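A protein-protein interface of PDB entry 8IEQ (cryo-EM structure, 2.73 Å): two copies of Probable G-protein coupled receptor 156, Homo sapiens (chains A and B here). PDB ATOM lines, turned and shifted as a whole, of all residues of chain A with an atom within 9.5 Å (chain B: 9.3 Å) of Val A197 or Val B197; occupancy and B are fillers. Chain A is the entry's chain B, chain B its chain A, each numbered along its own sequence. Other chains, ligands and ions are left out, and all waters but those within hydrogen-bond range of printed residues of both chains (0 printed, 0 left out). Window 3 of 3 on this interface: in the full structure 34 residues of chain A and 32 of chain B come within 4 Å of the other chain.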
ATOM      1  N   ILE A 194       7.107 -10.234 -33.525  1.00  0.00           N
ATOM      2  CA  ILE A 194       6.109 -11.109 -32.921  1.00  0.00           C
ATOM      3  C   ILE A 194       5.460 -10.382 -31.755  1.00  0.00           C
ATOM      4  O   ILE A 194       6.150  -9.832 -30.889  1.00  0.00           O
ATOM      5  CB  ILE A 194       6.718 -12.452 -32.463  1.00  0.00           C
ATOM      6  CG1 ILE A 194       7.967 -12.239 -31.598  1.00  0.00           C
ATOM      7  CG2 ILE A 194       7.058 -13.311 -33.664  1.00  0.00           C
ATOM      8  CD1 ILE A 194       8.446 -13.495 -30.898  1.00  0.00           C
ATOM      9  N   LEU A 195       4.132 -10.355 -31.752  1.00  0.00           N
ATOM     10  CA  LEU A 195       3.348  -9.997 -30.580  1.00  0.00           C
ATOM     11  C   LEU A 195       2.721 -11.279 -30.056  1.00  0.00           C
ATOM     12  O   LEU A 195       2.164 -12.061 -30.832  1.00  0.00           O
ATOM     13  CB  LEU A 195       2.295  -8.932 -30.911  1.00  0.00           C
ATOM     14  CG  LEU A 195       1.168  -9.189 -31.920  1.00  0.00           C
ATOM     15  CD1 LEU A 195      -0.052  -9.869 -31.294  1.00  0.00           C
ATOM     16  CD2 LEU A 195       0.758  -7.884 -32.590  1.00  0.00           C
ATOM     17  N   SER A 196       2.868 -11.521 -28.757  1.00  0.00           N
ATOM     18  CA  SER A 196       2.476 -12.798 -28.183  1.00  0.00           C
ATOM     19  C   SER A 196       2.084 -12.605 -26.729  1.00  0.00           C
ATOM     20  O   SER A 196       2.650 -11.760 -26.031  1.00  0.00           O
ATOM     21  CB  SER A 196       3.613 -13.821 -28.286  1.00  0.00           C
ATOM     22  OG  SER A 196       4.526 -13.675 -27.213  1.00  0.00           O
ATOM     23  N   VAL A 197       1.108 -13.395 -26.288  1.00  0.00           N
ATOM     24  CA  VAL A 197       0.689 -13.455 -24.893  1.00  0.00           C
ATOM     25  C   VAL A 197       0.944 -14.871 -24.400  1.00  0.00           C
ATOM     26  O   VAL A 197       0.471 -15.841 -25.005  1.00  0.00           O
ATOM     27  CB  VAL A 197      -0.788 -13.051 -24.720  1.00  0.00           C
ATOM     28  CG1 VAL A 197      -0.963 -11.570 -25.009  1.00  0.00           C
ATOM     29  CG2 VAL A 197      -1.718 -13.882 -25.612  1.00  0.00           C
ATOM     30  N   SER A 198       1.706 -14.990 -23.316  1.00  0.00           N
ATOM     31  CA  SER A 198       2.143 -16.274 -22.787  1.00  0.00           C
ATOM     32  C   SER A 198       1.509 -16.500 -21.425  1.00  0.00           C
ATOM     33  O   SER A 198       1.584 -15.631 -20.549  1.00  0.00           O
ATOM     34  CB  SER A 198       3.668 -16.333 -22.680  1.00  0.00           C
ATOM     35  OG  SER A 198       4.270 -16.233 -23.959  1.00  0.00           O
ATOM     36  N   MET A 199       0.890 -17.665 -21.254  1.00  0.00           N
ATOM     37  CA  MET A 199       0.216 -18.052 -20.017  1.00  0.00           C
ATOM     38  C   MET A 199       0.963 -19.256 -19.456  1.00  0.00           C
ATOM     39  O   MET A 199       0.598 -20.405 -19.714  1.00  0.00           O
ATOM     40  CB  MET A 199      -1.256 -18.366 -20.281  1.00  0.00           C
ATOM     41  CG  MET A 199      -2.083 -17.149 -20.668  1.00  0.00           C
ATOM     42  SD  MET A 199      -3.805 -17.544 -21.031  1.00  0.00           S
ATOM     43  CE  MET A 199      -3.689 -18.017 -22.755  1.00  0.00           C
ATOM     44  N   THR A 200       2.013 -18.985 -18.687  1.00  0.00           N
ATOM     45  CA  THR A 200       2.830 -20.029 -18.093  1.00  0.00           C
ATOM     46  C   THR A 200       2.294 -20.404 -16.716  1.00  0.00           C
ATOM     47  O   THR A 200       1.539 -19.656 -16.090  1.00  0.00           O
ATOM     48  CB  THR A 200       4.290 -19.578 -17.984  1.00  0.00           C
ATOM     49  OG1 THR A 200       5.129 -20.715 -17.744  1.00  0.00           O
ATOM     50  CG2 THR A 200       4.470 -18.568 -16.853  1.00  0.00           C
ATOM     51  N   SER A 207       1.096 -17.347 -13.890  1.00  0.00           N
ATOM     52  CA  SER A 207       1.431 -15.985 -14.284  1.00  0.00           C
ATOM     53  C   SER A 207       1.244 -15.837 -15.786  1.00  0.00           C
ATOM     54  O   SER A 207       1.386 -16.802 -16.542  1.00  0.00           O
ATOM     55  CB  SER A 207       2.869 -15.622 -13.892  1.00  0.00           C
ATOM     56  OG  SER A 207       3.772 -16.656 -14.247  1.00  0.00           O
ATOM     57  N   CYS A 208       0.923 -14.614 -16.208  1.00  0.00           N
ATOM     58  CA  CYS A 208       0.675 -14.290 -17.607  1.00  0.00           C
ATOM     59  C   CYS A 208       1.541 -13.108 -18.012  1.00  0.00           C
ATOM     60  O   CYS A 208       1.706 -12.157 -17.243  1.00  0.00           O
ATOM     61  CB  CYS A 208      -0.801 -13.961 -17.848  1.00  0.00           C
ATOM     62  SG  CYS A 208      -1.949 -15.252 -17.316  1.00  0.00           S
ATOM     63  N   THR A 209       2.089 -13.174 -19.224  1.00  0.00           N
ATOM     64  CA  THR A 209       2.950 -12.132 -19.762  1.00  0.00           C
ATOM     65  C   THR A 209       2.521 -11.800 -21.184  1.00  0.00           C
ATOM     66  O   THR A 209       1.956 -12.637 -21.893  1.00  0.00           O
ATOM     67  CB  THR A 209       4.426 -12.557 -19.759  1.00  0.00           C
ATOM     68  OG1 THR A 209       4.560 -13.842 -20.377  1.00  0.00           O
ATOM     69  CG2 THR A 209       4.962 -12.621 -18.338  1.00  0.00           C
ATOM     70  N   SER A 210       2.795 -10.560 -21.590  1.00  0.00           N
ATOM     71  CA  SER A 210       2.467 -10.074 -22.931  1.00  0.00           C
ATOM     72  C   SER A 210       3.662  -9.262 -23.418  1.00  0.00           C
ATOM     73  O   SER A 210       3.858  -8.122 -22.986  1.00  0.00           O
ATOM     74  CB  SER A 210       1.193  -9.238 -22.922  1.00  0.00           C
ATOM     75  OG  SER A 210       0.143  -9.919 -22.257  1.00  0.00           O
ATOM     76  N   THR A 211       4.452  -9.851 -24.313  1.00  0.00           N
ATOM     77  CA  THR A 211       5.681  -9.248 -24.808  1.00  0.00           C
ATOM     78  C   THR A 211       5.633  -9.139 -26.324  1.00  0.00           C
ATOM     79  O   THR A 211       5.100 -10.019 -27.006  1.00  0.00           O
ATOM     80  CB  THR A 211       6.906 -10.071 -24.395  1.00  0.00           C
ATOM     81  OG1 THR A 211       6.768 -11.414 -24.875  1.00  0.00           O
ATOM     82  CG2 THR A 211       7.057 -10.087 -22.881  1.00  0.00           C
ATOM     83  N   SER A 212       6.190  -8.045 -26.842  1.00  0.00           N
ATOM     84  CA  SER A 212       6.365  -7.837 -28.272  1.00  0.00           C
ATOM     85  C   SER A 212       7.813  -7.448 -28.523  1.00  0.00           C
ATOM     86  O   SER A 212       8.334  -6.539 -27.869  1.00  0.00           O
ATOM     87  CB  SER A 212       5.420  -6.755 -28.801  1.00  0.00           C
ATOM     88  OG  SER A 212       5.286  -6.836 -30.209  1.00  0.00           O
ATOM     89  N   ILE B 194       4.383 -24.004 -20.950  1.00  0.00           N
ATOM     90  CA  ILE B 194       4.227 -22.776 -21.721  1.00  0.00           C
ATOM     91  C   ILE B 194       3.176 -23.030 -22.790  1.00  0.00           C
ATOM     92  O   ILE B 194       3.401 -23.809 -23.723  1.00  0.00           O
ATOM     93  CB  ILE B 194       5.557 -22.327 -22.342  1.00  0.00           C
ATOM     94  CG1 ILE B 194       6.533 -21.868 -21.253  1.00  0.00           C
ATOM     95  CG2 ILE B 194       5.329 -21.220 -23.373  1.00  0.00           C
ATOM     96  CD1 ILE B 194       6.285 -20.462 -20.742  1.00  0.00           C
ATOM     97  N   LEU B 195       2.026 -22.376 -22.652  1.00  0.00           N
ATOM     98  CA  LEU B 195       1.006 -22.323 -23.689  1.00  0.00           C
ATOM     99  C   LEU B 195       0.787 -20.862 -24.043  1.00  0.00           C
ATOM    100  O   LEU B 195       0.647 -20.018 -23.151  1.00  0.00           O
ATOM    101  CB  LEU B 195      -0.293 -23.001 -23.229  1.00  0.00           C
ATOM    102  CG  LEU B 195      -1.067 -22.451 -22.025  1.00  0.00           C
ATOM    103  CD1 LEU B 195      -2.103 -21.401 -22.424  1.00  0.00           C
ATOM    104  CD2 LEU B 195      -1.732 -23.592 -21.266  1.00  0.00           C
ATOM    105  N   SER B 196       0.798 -20.558 -25.337  1.00  0.00           N
ATOM    106  CA  SER B 196       0.783 -19.172 -25.776  1.00  0.00           C
ATOM    107  C   SER B 196       0.283 -19.101 -27.209  1.00  0.00           C
ATOM    108  O   SER B 196       0.258 -20.102 -27.931  1.00  0.00           O
ATOM    109  CB  SER B 196       2.176 -18.542 -25.669  1.00  0.00           C
ATOM    110  OG  SER B 196       3.060 -19.099 -26.627  1.00  0.00           O
ATOM    111  N   VAL B 197      -0.120 -17.897 -27.605  1.00  0.00           N
ATOM    112  CA  VAL B 197      -0.511 -17.589 -28.973  1.00  0.00           C
ATOM    113  C   VAL B 197       0.282 -16.371 -29.421  1.00  0.00           C
ATOM    114  O   VAL B 197       0.333 -15.358 -28.714  1.00  0.00           O
ATOM    115  CB  VAL B 197      -2.030 -17.340 -29.101  1.00  0.00           C
ATOM    116  CG1 VAL B 197      -2.799 -18.618 -28.805  1.00  0.00           C
ATOM    117  CG2 VAL B 197      -2.492 -16.206 -28.183  1.00  0.00           C
ATOM    118  N   SER B 198       0.915 -16.478 -30.589  1.00  0.00           N
ATOM    119  CA  SER B 198       1.782 -15.433 -31.109  1.00  0.00           C
ATOM    120  C   SER B 198       1.408 -15.132 -32.551  1.00  0.00           C
ATOM    121  O   SER B 198       1.120 -16.044 -33.331  1.00  0.00           O
ATOM    122  CB  SER B 198       3.257 -15.845 -31.033  1.00  0.00           C
ATOM    123  OG  SER B 198       3.566 -16.811 -32.022  1.00  0.00           O
ATOM    124  N   MET B 199       1.415 -13.846 -32.894  1.00  0.00           N
ATOM    125  CA  MET B 199       1.185 -13.376 -34.254  1.00  0.00           C
ATOM    126  C   MET B 199       2.522 -12.912 -34.813  1.00  0.00           C
ATOM    127  O   MET B 199       3.150 -12.009 -34.250  1.00  0.00           O
ATOM    128  CB  MET B 199       0.151 -12.247 -34.268  1.00  0.00           C
ATOM    129  CG  MET B 199      -0.015 -11.495 -35.595  1.00  0.00           C
ATOM    130  SD  MET B 199      -1.034 -10.021 -35.411  1.00  0.00           S
ATOM    131  CE  MET B 199      -2.655 -10.683 -35.784  1.00  0.00           C
ATOM    132  N   THR B 200       2.949 -13.521 -35.914  1.00  0.00           N
ATOM    133  CA  THR B 200       4.221 -13.201 -36.549  1.00  0.00           C
ATOM    134  C   THR B 200       3.978 -12.173 -37.645  1.00  0.00           C
ATOM    135  O   THR B 200       3.120 -12.378 -38.511  1.00  0.00           O
ATOM    136  CB  THR B 200       4.877 -14.453 -37.131  1.00  0.00           C
ATOM    137  OG1 THR B 200       4.120 -14.911 -38.257  1.00  0.00           O
ATOM    138  CG2 THR B 200       4.947 -15.562 -36.091  1.00  0.00           C
ATOM    139  N   SER B 207       0.927 -14.496 -39.668  1.00  0.00           N
ATOM    140  CA  SER B 207       0.647 -15.878 -39.305  1.00  0.00           C
ATOM    141  C   SER B 207       0.454 -15.978 -37.800  1.00  0.00           C
ATOM    142  O   SER B 207       1.201 -15.369 -37.027  1.00  0.00           O
ATOM    143  CB  SER B 207       1.779 -16.813 -39.747  1.00  0.00           C
ATOM    144  OG  SER B 207       1.402 -18.171 -39.607  1.00  0.00           O
ATOM    145  N   CYS B 208      -0.552 -16.749 -37.391  1.00  0.00           N
ATOM    146  CA  CYS B 208      -0.868 -16.982 -35.989  1.00  0.00           C
ATOM    147  C   CYS B 208      -0.657 -18.455 -35.674  1.00  0.00           C
ATOM    148  O   CYS B 208      -1.102 -19.324 -36.431  1.00  0.00           O
ATOM    149  CB  CYS B 208      -2.308 -16.573 -35.671  1.00  0.00           C
ATOM    150  SG  CYS B 208      -2.632 -14.804 -35.843  1.00  0.00           S
ATOM    151  N   THR B 209       0.023 -18.729 -34.562  1.00  0.00           N
ATOM    152  CA  THR B 209       0.313 -20.087 -34.127  1.00  0.00           C
ATOM    153  C   THR B 209      -0.014 -20.228 -32.648  1.00  0.00           C
ATOM    154  O   THR B 209       0.158 -19.282 -31.873  1.00  0.00           O
ATOM    155  CB  THR B 209       1.785 -20.449 -34.373  1.00  0.00           C
ATOM    156  OG1 THR B 209       2.185 -19.979 -35.666  1.00  0.00           O
ATOM    157  CG2 THR B 209       1.990 -21.957 -34.302  1.00  0.00           C
ATOM    158  N   SER B 210      -0.495 -21.410 -32.268  1.00  0.00           N
ATOM    159  CA  SER B 210      -0.799 -21.750 -30.882  1.00  0.00           C
ATOM    160  C   SER B 210       0.020 -22.981 -30.515  1.00  0.00           C
ATOM    161  O   SER B 210      -0.194 -24.061 -31.074  1.00  0.00           O
ATOM    162  CB  SER B 210      -2.293 -22.005 -30.695  1.00  0.00           C
ATOM    163  OG  SER B 210      -3.063 -20.944 -31.232  1.00  0.00           O
ATOM    164  N   THR B 211       0.950 -22.815 -29.578  1.00  0.00           N
ATOM    165  CA  THR B 211       1.870 -23.871 -29.173  1.00  0.00           C
ATOM    166  C   THR B 211       1.785 -24.072 -27.669  1.00  0.00           C
ATOM    167  O   THR B 211       1.804 -23.100 -26.907  1.00  0.00           O
ATOM    168  CB  THR B 211       3.308 -23.533 -29.574  1.00  0.00           C
ATOM    169  OG1 THR B 211       3.654 -22.234 -29.076  1.00  0.00           O
ATOM    170  CG2 THR B 211       3.462 -23.550 -31.087  1.00  0.00           C
ATOM    171  N   SER B 212       1.690 -25.332 -27.250  1.00  0.00           N
ATOM    172  CA  SER B 212       1.723 -25.722 -25.843  1.00  0.00           C
ATOM    173  C   SER B 212       2.993 -26.542 -25.639  1.00  0.00           C
ATOM    174  O   SER B 212       3.021 -27.741 -25.932  1.00  0.00           O
ATOM    175  CB  SER B 212       0.474 -26.509 -25.460  1.00  0.00           C
ATOM    176  OG  SER B 212       0.334 -26.593 -24.052  1.00  0.00           O
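The backbone NH (N) of Met B199 lies within hydrogen-bond range of the backbone carbonyl oxygen (O) of Leu A195, at 2.8 Å.
The backbone carbonyl oxygen (O) of Leu B195 is in hydrogen-bond range of the backbone NH (N) of Met A199.
The backbone carbonyl oxygen (O) of Val B197 sits at hydrogen-bond distance from the backbone NH (N) of Val A197, at 3.2 Å.
The backbone carbonyl oxygen of Ser A196 is in hydrogen-bond range of the backbone NH of Thr A211, at 3.1 Å.
O of Ile A194 lies within hydrogen-bond range of OG of Ser A212, 3.2 Å away.
The backbone NH (N) of Thr B200 sits at hydrogen-bond distance from the backbone carbonyl oxygen (O) of Ser B207, 2.8 Å away.
The backbone NH (N) of Ser B196 lies within hydrogen-bond range of the backbone carbonyl oxygen (O) of Thr B211 (3.2 Å).
N of Ser A198 is in hydrogen-bond range of O of Thr A209 (2.8 Å).
The backbone NH (N) of Thr B209 lies within hydrogen-bond range of the backbone carbonyl oxygen (O) of Ser B198, 3.2 Å away.
Ile A194 touches Met B199 (CA to O, 3.4 Å).
Ile A194 touches Thr B200 (CG2 to CG2, 3.9 Å).
Leu A195 touches Ser B198.
O of Val B197 touches CA of Ser A196 (3.4 Å).
Ser A196 touches Ser B198 (CB to CB, 3.4 Å).
Ser B196 touches Val A197 (CB to O, 3.3 Å).
OG of Ser A198 touches CB of Ser B196 (3.6 Å).
OG1 of Thr A200 touches CD1 of Ile B194, at 3.2 Å.
Ser A196 touches just these residues of chain B: Val B197 and Ser B198.
Of chain B, only Ser B196 (3.3 Å) and Val B197 (3.2 Å) come within 4 Å of Val A197.
Printed residues of chain B within 4 Å of Ser A198: Ser B196.
Printed residues of chain B within 4 Å of Thr A200: Ile B194 (3.2 Å).
Cys A208 touches none of the printed residues of chain B.
Of the printed residues of chain A, Ile B194 touches Thr A200.
Of the printed residues of chain A, Ser B196 touches Val A197 (3.3 Å) and Ser A198 (3.6 Å).
Val B197 touches two residues of chain A.
The nearest residue of chain B that does not touch Val A197 is Leu B195 (4.6 Å).
Of the 13 printed residues of chain A, 7 touch a printed residue of chain B.
Hydrophobic or aromatic side chains of chain A within 4 Å of the printed part of chain B: Ile A194, Leu A195, Val A197 and Met A199.
Of the 13 printed residues of chain B, 7 touch a printed residue of chain A.
Among the printed residues, 11 pairs touch across the chains.
Among the printed residues, no Asp or Glu carboxylate lies within 4 Å of a Lys or Arg side-chain nitrogen of the other chain.
Leu A195 touches Ser B198, but with the chains exchanged Ser A198 does not touch Leu B195 (4.01 Å).
Leu A195 touches Met B199, and with the chains exchanged Met A199 touches Leu B195.
Ser A196 touches Val B197, and with the chains exchanged Val A197 touches Ser B196.
Val A197 touches its own counterpart, Val B197.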
